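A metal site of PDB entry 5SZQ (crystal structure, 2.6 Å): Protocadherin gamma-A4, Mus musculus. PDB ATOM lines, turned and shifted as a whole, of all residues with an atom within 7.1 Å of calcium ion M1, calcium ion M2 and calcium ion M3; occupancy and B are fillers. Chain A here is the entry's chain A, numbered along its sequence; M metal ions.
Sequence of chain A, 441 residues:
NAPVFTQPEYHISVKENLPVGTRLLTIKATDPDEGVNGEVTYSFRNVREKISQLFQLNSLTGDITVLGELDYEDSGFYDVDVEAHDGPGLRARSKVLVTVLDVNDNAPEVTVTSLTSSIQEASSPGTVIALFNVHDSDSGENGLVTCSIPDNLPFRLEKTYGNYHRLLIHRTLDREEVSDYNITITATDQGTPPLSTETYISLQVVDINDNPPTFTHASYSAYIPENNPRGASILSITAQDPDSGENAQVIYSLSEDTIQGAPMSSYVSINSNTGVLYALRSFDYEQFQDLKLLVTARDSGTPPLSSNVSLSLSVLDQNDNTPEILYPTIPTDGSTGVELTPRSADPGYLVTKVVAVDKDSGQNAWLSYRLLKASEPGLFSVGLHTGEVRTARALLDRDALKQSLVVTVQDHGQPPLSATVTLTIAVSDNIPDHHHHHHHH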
ATOM      1  N   GLU A  16       4.838  17.377   0.635  1.00  0.00           N
ATOM      2  CA  GLU A  16       5.502  18.451  -0.105  1.00  0.00           C
ATOM      3  C   GLU A  16       7.017  18.296  -0.160  1.00  0.00           C
ATOM      4  O   GLU A  16       7.653  18.836  -1.060  1.00  0.00           O
ATOM      5  CB  GLU A  16       5.142  19.806   0.518  1.00  0.00           C
ATOM      6  CG  GLU A  16       5.672  19.974   1.937  1.00  0.00           C
ATOM      7  CD  GLU A  16       5.514  21.392   2.437  1.00  0.00           C
ATOM      8  OE1 GLU A  16       5.446  22.310   1.599  1.00  0.00           O
ATOM      9  OE2 GLU A  16       5.440  21.596   3.674  1.00  0.00           O
ATOM     10  N   ASN A  17       7.600  17.541   0.773  1.00  0.00           N
ATOM     11  CA  ASN A  17       9.047  17.417   0.878  1.00  0.00           C
ATOM     12  C   ASN A  17       9.624  16.336  -0.027  1.00  0.00           C
ATOM     13  O   ASN A  17      10.766  15.911   0.194  1.00  0.00           O
ATOM     14  CB  ASN A  17       9.455  17.135   2.326  1.00  0.00           C
ATOM     15  CG  ASN A  17       9.060  15.736   2.778  1.00  0.00           C
ATOM     16  OD1 ASN A  17       8.082  15.160   2.297  1.00  0.00           O
ATOM     17  ND2 ASN A  17       9.822  15.166   3.714  1.00  0.00           N
ATOM     18  N   GLU A  69      10.687  21.195  -6.706  1.00  0.00           N
ATOM     19  CA  GLU A  69      10.161  20.960  -5.367  1.00  0.00           C
ATOM     20  C   GLU A  69       8.765  21.554  -5.217  1.00  0.00           C
ATOM     21  O   GLU A  69       8.519  22.704  -5.594  1.00  0.00           O
ATOM     22  CB  GLU A  69      11.115  21.555  -4.324  1.00  0.00           C
ATOM     23  CG  GLU A  69      10.628  21.452  -2.876  1.00  0.00           C
ATOM     24  CD  GLU A  69      10.879  20.084  -2.261  1.00  0.00           C
ATOM     25  OE1 GLU A  69      11.042  19.103  -3.022  1.00  0.00           O
ATOM     26  OE2 GLU A  69      10.903  20.000  -1.007  1.00  0.00           O
ATOM     27  N   LEU A  70       7.859  20.747  -4.667  1.00  0.00           N
ATOM     28  CA  LEU A  70       6.485  21.168  -4.458  1.00  0.00           C
ATOM     29  C   LEU A  70       6.352  21.789  -3.084  1.00  0.00           C
ATOM     30  O   LEU A  70       6.688  21.162  -2.066  1.00  0.00           O
ATOM     31  CB  LEU A  70       5.526  19.981  -4.597  1.00  0.00           C
ATOM     32  CG  LEU A  70       5.730  19.071  -5.820  1.00  0.00           C
ATOM     33  CD1 LEU A  70       4.734  17.922  -5.826  1.00  0.00           C
ATOM     34  CD2 LEU A  70       5.623  19.864  -7.111  1.00  0.00           C
ATOM     35  N   ASP A  71       5.868  23.020  -3.030  1.00  0.00           N
ATOM     36  CA  ASP A  71       5.661  23.727  -1.778  1.00  0.00           C
ATOM     37  C   ASP A  71       4.161  23.737  -1.510  1.00  0.00           C
ATOM     38  O   ASP A  71       3.400  24.316  -2.294  1.00  0.00           O
ATOM     39  CB  ASP A  71       6.224  25.141  -1.854  1.00  0.00           C
ATOM     40  CG  ASP A  71       6.475  25.736  -0.487  1.00  0.00           C
ATOM     41  OD1 ASP A  71       7.016  25.021   0.383  1.00  0.00           O
ATOM     42  OD2 ASP A  71       6.120  26.918  -0.286  1.00  0.00           O
ATOM     43  N   TYR A  72       3.738  23.073  -0.427  1.00  0.00           N
ATOM     44  CA  TYR A  72       2.325  23.084  -0.066  1.00  0.00           C
ATOM     45  C   TYR A  72       1.828  24.512   0.089  1.00  0.00           C
ATOM     46  O   TYR A  72       0.703  24.839  -0.314  1.00  0.00           O
ATOM     47  CB  TYR A  72       2.093  22.293   1.226  1.00  0.00           C
ATOM     48  CG  TYR A  72       0.638  22.220   1.683  1.00  0.00           C
ATOM     49  CD1 TYR A  72      -0.103  21.065   1.495  1.00  0.00           C
ATOM     50  CD2 TYR A  72       0.021  23.294   2.319  1.00  0.00           C
ATOM     51  CE1 TYR A  72      -1.428  20.981   1.905  1.00  0.00           C
ATOM     52  CE2 TYR A  72      -1.295  23.224   2.735  1.00  0.00           C
ATOM     53  CZ  TYR A  72      -2.012  22.072   2.524  1.00  0.00           C
ATOM     54  OH  TYR A  72      -3.324  21.993   2.939  1.00  0.00           O
ATOM     55  N   GLU A  73       2.651  25.372   0.680  1.00  0.00           N
ATOM     56  CA  GLU A  73       2.290  26.773   0.876  1.00  0.00           C
ATOM     57  C   GLU A  73       2.127  27.531  -0.440  1.00  0.00           C
ATOM     58  O   GLU A  73       1.564  28.628  -0.431  1.00  0.00           O
ATOM     59  CB  GLU A  73       3.342  27.463   1.751  1.00  0.00           C
ATOM     60  CG  GLU A  73       3.305  27.042   3.212  1.00  0.00           C
ATOM     61  CD  GLU A  73       3.765  25.619   3.439  1.00  0.00           C
ATOM     62  OE1 GLU A  73       4.836  25.257   2.907  1.00  0.00           O
ATOM     63  OE2 GLU A  73       3.059  24.863   4.134  1.00  0.00           O
ATOM     64  N   ASP A  74       2.608  26.967  -1.549  1.00  0.00           N
ATOM     65  CA  ASP A  74       2.400  27.579  -2.858  1.00  0.00           C
ATOM     66  C   ASP A  74       1.109  27.078  -3.503  1.00  0.00           C
ATOM     67  O   ASP A  74       0.308  27.880  -3.999  1.00  0.00           O
ATOM     68  CB  ASP A  74       3.596  27.287  -3.767  1.00  0.00           C
ATOM     69  CG  ASP A  74       3.530  28.047  -5.084  1.00  0.00           C
ATOM     70  OD1 ASP A  74       3.071  29.219  -5.088  1.00  0.00           O
ATOM     71  OD2 ASP A  74       3.940  27.476  -6.126  1.00  0.00           O
ATOM     72  N   LEU A 101       0.550  17.119   0.404  1.00  0.00           N
ATOM     73  CA  LEU A 101       0.310  17.103   1.837  1.00  0.00           C
ATOM     74  C   LEU A 101       1.224  18.099   2.522  1.00  0.00           C
ATOM     75  O   LEU A 101       2.307  18.441   2.032  1.00  0.00           O
ATOM     76  CB  LEU A 101       0.545  15.698   2.409  1.00  0.00           C
ATOM     77  CG  LEU A 101      -0.251  14.569   1.743  1.00  0.00           C
ATOM     78  CD1 LEU A 101       0.052  13.234   2.397  1.00  0.00           C
ATOM     79  CD2 LEU A 101      -1.750  14.857   1.750  1.00  0.00           C
ATOM     80  N   ASP A 102       0.773  18.596   3.671  1.00  0.00           N
ATOM     81  CA  ASP A 102       1.503  19.621   4.415  1.00  0.00           C
ATOM     82  C   ASP A 102       2.549  18.969   5.309  1.00  0.00           C
ATOM     83  O   ASP A 102       2.254  18.018   6.041  1.00  0.00           O
ATOM     84  CB  ASP A 102       0.532  20.451   5.247  1.00  0.00           C
ATOM     85  CG  ASP A 102       1.246  21.407   6.174  1.00  0.00           C
ATOM     86  OD1 ASP A 102       0.681  21.734   7.244  1.00  0.00           O
ATOM     87  OD2 ASP A 102       2.378  21.825   5.851  1.00  0.00           O
ATOM     88  N   VAL A 103       3.775  19.489   5.240  1.00  0.00           N
ATOM     89  CA  VAL A 103       4.866  19.084   6.113  1.00  0.00           C
ATOM     90  C   VAL A 103       5.277  20.293   6.934  1.00  0.00           C
ATOM     91  O   VAL A 103       5.415  21.397   6.386  1.00  0.00           O
ATOM     92  CB  VAL A 103       6.062  18.527   5.317  1.00  0.00           C
ATOM     93  CG1 VAL A 103       7.214  18.190   6.253  1.00  0.00           C
ATOM     94  CG2 VAL A 103       5.648  17.303   4.522  1.00  0.00           C
ATOM     95  N   ASN A 104       5.449  20.098   8.235  1.00  0.00           N
ATOM     96  CA  ASN A 104       5.860  21.189   9.128  1.00  0.00           C
ATOM     97  C   ASN A 104       7.322  21.519   8.842  1.00  0.00           C
ATOM     98  O   ASN A 104       8.245  21.071   9.521  1.00  0.00           O
ATOM     99  CB  ASN A 104       5.647  20.795  10.589  1.00  0.00           C
ATOM    100  CG  ASN A 104       5.968  21.915  11.552  1.00  0.00           C
ATOM    101  OD1 ASN A 104       5.987  23.081  11.173  1.00  0.00           O
ATOM    102  ND2 ASN A 104       6.233  21.568  12.809  1.00  0.00           N
ATOM    103  N   ASP A 105       7.528  22.341   7.814  1.00  0.00           N
ATOM    104  CA  ASP A 105       8.863  22.764   7.408  1.00  0.00           C
ATOM    105  C   ASP A 105       9.082  24.273   7.533  1.00  0.00           C
ATOM    106  O   ASP A 105      10.074  24.785   7.017  1.00  0.00           O
ATOM    107  CB  ASP A 105       9.158  22.316   5.969  1.00  0.00           C
ATOM    108  CG  ASP A 105       8.174  22.907   4.965  1.00  0.00           C
ATOM    109  OD1 ASP A 105       8.024  22.292   3.887  1.00  0.00           O
ATOM    110  OD2 ASP A 105       7.566  23.959   5.245  1.00  0.00           O
ATOM    111  N   ASN A 106       8.174  24.992   8.207  1.00  0.00           N
ATOM    112  CA  ASN A 106       8.339  26.422   8.434  1.00  0.00           C
ATOM    113  C   ASN A 106       8.160  26.699   9.921  1.00  0.00           C
ATOM    114  O   ASN A 106       7.054  26.577  10.447  1.00  0.00           O
ATOM    115  CB  ASN A 106       7.330  27.241   7.610  1.00  0.00           C
ATOM    116  CG  ASN A 106       7.735  27.372   6.153  1.00  0.00           C
ATOM    117  OD1 ASN A 106       8.897  27.173   5.789  1.00  0.00           O
ATOM    118  ND2 ASN A 106       6.773  27.703   5.308  1.00  0.00           N
ATOM    119  N   ALA A 107       9.256  27.059  10.599  1.00  0.00           N
ATOM    120  CA  ALA A 107       9.154  27.448  11.990  1.00  0.00           C
ATOM    121  C   ALA A 107       8.382  28.769  12.109  1.00  0.00           C
ATOM    122  O   ALA A 107       8.393  29.578  11.172  1.00  0.00           O
ATOM    123  CB  ALA A 107      10.537  27.584  12.610  1.00  0.00           C
ATOM    124  N   PRO A 108       7.693  28.998  13.226  1.00  0.00           N
ATOM    125  CA  PRO A 108       6.908  30.222  13.365  1.00  0.00           C
ATOM    126  C   PRO A 108       7.769  31.469  13.285  1.00  0.00           C
ATOM    127  O   PRO A 108       8.922  31.486  13.729  1.00  0.00           O
ATOM    128  CB  PRO A 108       6.253  30.078  14.740  1.00  0.00           C
ATOM    129  CG  PRO A 108       7.055  29.036  15.445  1.00  0.00           C
ATOM    130  CD  PRO A 108       7.516  28.102  14.374  1.00  0.00           C
ATOM    131  N   ASP A 136       2.563  31.892  11.231  1.00  0.00           N
ATOM    132  CA  ASP A 136       3.186  30.665  10.735  1.00  0.00           C
ATOM    133  C   ASP A 136       2.632  30.360   9.346  1.00  0.00           C
ATOM    134  O   ASP A 136       1.414  30.436   9.130  1.00  0.00           O
ATOM    135  CB  ASP A 136       2.936  29.494  11.687  1.00  0.00           C
ATOM    136  CG  ASP A 136       3.776  28.269  11.346  1.00  0.00           C
ATOM    137  OD1 ASP A 136       4.728  28.385  10.548  1.00  0.00           O
ATOM    138  OD2 ASP A 136       3.487  27.180  11.906  1.00  0.00           O
ATOM    139  N   SER A 137       3.522  30.011   8.418  1.00  0.00           N
ATOM    140  CA  SER A 137       3.127  29.736   7.051  1.00  0.00           C
ATOM    141  C   SER A 137       2.516  28.341   6.891  1.00  0.00           C
ATOM    142  O   SER A 137       1.776  28.110   5.932  1.00  0.00           O
ATOM    143  CB  SER A 137       4.337  29.888   6.118  1.00  0.00           C
ATOM    144  OG  SER A 137       4.847  31.209   6.180  1.00  0.00           O
ATOM    145  N   ASP A 138       2.810  27.425   7.802  1.00  0.00           N
ATOM    146  CA  ASP A 138       2.288  26.070   7.685  1.00  0.00           C
ATOM    147  C   ASP A 138       0.793  26.045   7.999  1.00  0.00           C
ATOM    148  O   ASP A 138       0.211  27.013   8.500  1.00  0.00           O
ATOM    149  CB  ASP A 138       3.053  25.104   8.585  1.00  0.00           C
ATOM    150  CG  ASP A 138       4.488  24.899   8.142  1.00  0.00           C
ATOM    151  OD1 ASP A 138       4.690  24.286   7.068  1.00  0.00           O
ATOM    152  OD2 ASP A 138       5.406  25.336   8.868  1.00  0.00           O
ATOM    153  N   SER A 139       0.165  24.909   7.711  1.00  0.00           N
ATOM    154  CA  SER A 139      -1.279  24.748   7.821  1.00  0.00           C
ATOM    155  C   SER A 139      -1.634  23.738   8.900  1.00  0.00           C
ATOM    156  O   SER A 139      -0.789  22.949   9.351  1.00  0.00           O
ATOM    157  CB  SER A 139      -1.873  24.307   6.480  1.00  0.00           C
ATOM    158  OG  SER A 139      -1.268  25.014   5.406  1.00  0.00           O
ATOM    159  N   GLU A 141      -2.530  21.894  12.382  1.00  0.00           N
ATOM    160  CA  GLU A 141      -1.819  21.951  13.656  1.00  0.00           C
ATOM    161  C   GLU A 141      -0.353  22.329  13.473  1.00  0.00           C
ATOM    162  O   GLU A 141       0.264  22.825  14.419  1.00  0.00           O
ATOM    163  CB  GLU A 141      -1.931  20.619  14.401  1.00  0.00           C
ATOM    164  CG  GLU A 141      -3.253  20.420  15.125  1.00  0.00           C
ATOM    165  CD  GLU A 141      -3.236  19.214  16.048  1.00  0.00           C
ATOM    166  OE1 GLU A 141      -2.367  18.334  15.868  1.00  0.00           O
ATOM    167  OE2 GLU A 141      -4.082  19.161  16.966  1.00  0.00           O
ATOM    168  N   ASN A 142       0.208  22.100  12.281  1.00  0.00           N
ATOM    169  CA  ASN A 142       1.534  22.599  11.980  1.00  0.00           C
ATOM    170  C   ASN A 142       1.592  24.122  11.955  1.00  0.00           C
ATOM    171  O   ASN A 142       2.686  24.683  11.962  1.00  0.00           O
ATOM    172  CB  ASN A 142       2.029  22.051  10.629  1.00  0.00           C
ATOM    173  CG  ASN A 142       1.982  20.533  10.537  1.00  0.00           C
ATOM    174  OD1 ASN A 142       1.915  19.835  11.550  1.00  0.00           O
ATOM    175  ND2 ASN A 142       2.028  20.014   9.311  1.00  0.00           N
ATOM    176  N   GLY A 143       0.432  24.790  11.920  1.00  0.00           N
ATOM    177  CA  GLY A 143       0.365  26.228  11.788  1.00  0.00           C
ATOM    178  C   GLY A 143      -0.083  26.951  13.048  1.00  0.00           C
ATOM    179  O   GLY A 143       0.215  28.139  13.214  1.00  0.00           O
ATOM    180  N   LEU A 144      -0.818  26.265  13.924  1.00  0.00           N
ATOM    181  CA  LEU A 144      -1.130  26.839  15.221  1.00  0.00           C
ATOM    182  C   LEU A 144       0.148  27.031  16.026  1.00  0.00           C
ATOM    183  O   LEU A 144       1.115  26.287  15.860  1.00  0.00           O
ATOM    184  CB  LEU A 144      -2.121  25.951  15.976  1.00  0.00           C
ATOM    185  CG  LEU A 144      -3.520  25.794  15.377  1.00  0.00           C
ATOM    186  CD1 LEU A 144      -4.410  24.995  16.317  1.00  0.00           C
ATOM    187  CD2 LEU A 144      -4.155  27.152  15.062  1.00  0.00           C
ATOM    188  N   ASP A 189       5.656  25.431  17.926  1.00  0.00           N
ATOM    189  CA  ASP A 189       4.734  24.868  16.952  1.00  0.00           C
ATOM    190  C   ASP A 189       4.032  23.666  17.539  1.00  0.00           C
ATOM    191  O   ASP A 189       4.585  22.938  18.372  1.00  0.00           O
ATOM    192  CB  ASP A 189       5.491  24.473  15.681  1.00  0.00           C
ATOM    193  CG  ASP A 189       4.593  24.274  14.502  1.00  0.00           C
ATOM    194  OD1 ASP A 189       3.384  24.073  14.709  1.00  0.00           O
ATOM    195  OD2 ASP A 189       5.102  24.316  13.363  1.00  0.00           O
ATOM    196  N   GLN A 190       2.792  23.428  17.089  1.00  0.00           N
ATOM    197  CA  GLN A 190       2.001  22.304  17.563  1.00  0.00           C
ATOM    198  C   GLN A 190       2.154  21.061  16.686  1.00  0.00           C
ATOM    199  O   GLN A 190       1.909  19.944  17.163  1.00  0.00           O
ATOM    200  CB  GLN A 190       0.523  22.730  17.652  1.00  0.00           C
ATOM    201  CG  GLN A 190      -0.483  21.601  17.881  1.00  0.00           C
ATOM    202  CD  GLN A 190      -0.376  20.967  19.261  1.00  0.00           C
ATOM    203  OE1 GLN A 190      -0.086  21.647  20.244  1.00  0.00           O
ATOM    204  NE2 GLN A 190      -0.611  19.656  19.327  1.00  0.00           N
ATOM    205  N   GLY A 191       2.580  21.217  15.437  1.00  0.00           N
ATOM    206  CA  GLY A 191       2.718  20.067  14.555  1.00  0.00           C
ATOM    207  C   GLY A 191       3.994  19.279  14.830  1.00  0.00           C
ATOM    208  O   GLY A 191       5.055  19.845  15.107  1.00  0.00           O
ATOM    209  N   LEU A 195       8.454  22.780  15.880  1.00  0.00           N
ATOM    210  CA  LEU A 195       9.501  23.709  15.482  1.00  0.00           C
ATOM    211  C   LEU A 195       9.354  24.997  16.272  1.00  0.00           C
ATOM    212  O   LEU A 195       8.287  25.617  16.268  1.00  0.00           O
ATOM    213  CB  LEU A 195       9.455  24.015  13.986  1.00  0.00           C
ATOM    214  CG  LEU A 195      10.024  22.931  13.063  1.00  0.00           C
ATOM    215  CD1 LEU A 195      10.063  23.429  11.634  1.00  0.00           C
ATOM    216  CD2 LEU A 195      11.401  22.509  13.540  1.00  0.00           C
HETATM  217 CA    CA M   1       4.636  23.440   4.790  1.00  0.00          CA
HETATM  218 CA    CA M   2       7.028  24.133   2.507  1.00  0.00          CA
HETATM  219 CA    CA M   3       5.173  25.380  11.477  1.00  0.00          CA
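The backbone carbonyl oxygen (O) of Leu 195 sits close to the backbone NH (N) of Asp 189 (3.1 Å).
N of Gly 191 is in hydrogen-bond range of OD1 of Asp 189.
OE1 of Glu 16 sits close to N of Tyr 72 (2.8 Å).
O of Glu 16 lies close to O of Leu 70, 2.7 Å away.
The backbone NH (N) of Glu 16 sits at hydrogen-bond distance from the backbone carbonyl oxygen (O) of Leu 101, 3.1 Å away.
The backbone carbonyl oxygen (O) of Gly 191 sits at hydrogen-bond distance from the side-chain amide nitrogen (ND2) of Asn 104.
OD1 of Asp 102 lies within hydrogen-bond range of ND2 of Asn 142 (3.0 Å).
The side-chain carboxylate (OD1) of Asp 102 is in hydrogen-bond range of the backbone NH (N) of Ser 139 (3.3 Å).
Of the 28 residues printed, 4 come within 4 Å of calcium ion M2.
The nearest printed residue that does not touch calcium ion M2 is Tyr 72 (4.5 Å).
Calcium ion M1 is bound by the side-chain carboxylate (OE2) of Glu 73 (2.2 Å), the side-chain carboxylate (OE2) of Glu 16 (2.3 Å), the side-chain carboxylate (OD1) of Asp 138 (2.4 Å), the side-chain carboxylate (OE1) of Glu 73 (2.6 Å) and the backbone carbonyl oxygen (O) of Val 103 (2.7 Å).
Slightly farther from calcium ion M1 lies the side-chain carboxylate (OD2) of Asp 102 (3.0 Å).
Slightly farther from calcium ion M1 lies the side-chain carboxylate (OD2) of Asp 105 (3.0 Å).
Calcium ion M2 is bound by OD1 of Asp 71, at 2.3 Å.
The side-chain carboxylate (OE1) of Glu 73 is bound to calcium ion M2 (2.5 Å).
OD1 of Asp 105 binds calcium ion M2 (2.5 Å).
The side-chain carboxylate (OE1) of Glu 16 binds calcium ion M2 (2.6 Å).
Calcium ion M2 is bound by OD2 of Asp 105, at 2.8 Å.
Calcium ion M3 is bound by the side-chain carboxylate of Asp 189 (2.2 Å), the backbone carbonyl oxygen of Asn 106 (2.5 Å), the side-chain amide oxygen of Asn 104 (2.5 Å), the side-chain carboxylate of Asp 136 (2.5 Å), the side-chain carboxylate of Asp 138 (2.6 Å) and the backbone carbonyl oxygen of Asn 142 (2.6 Å).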
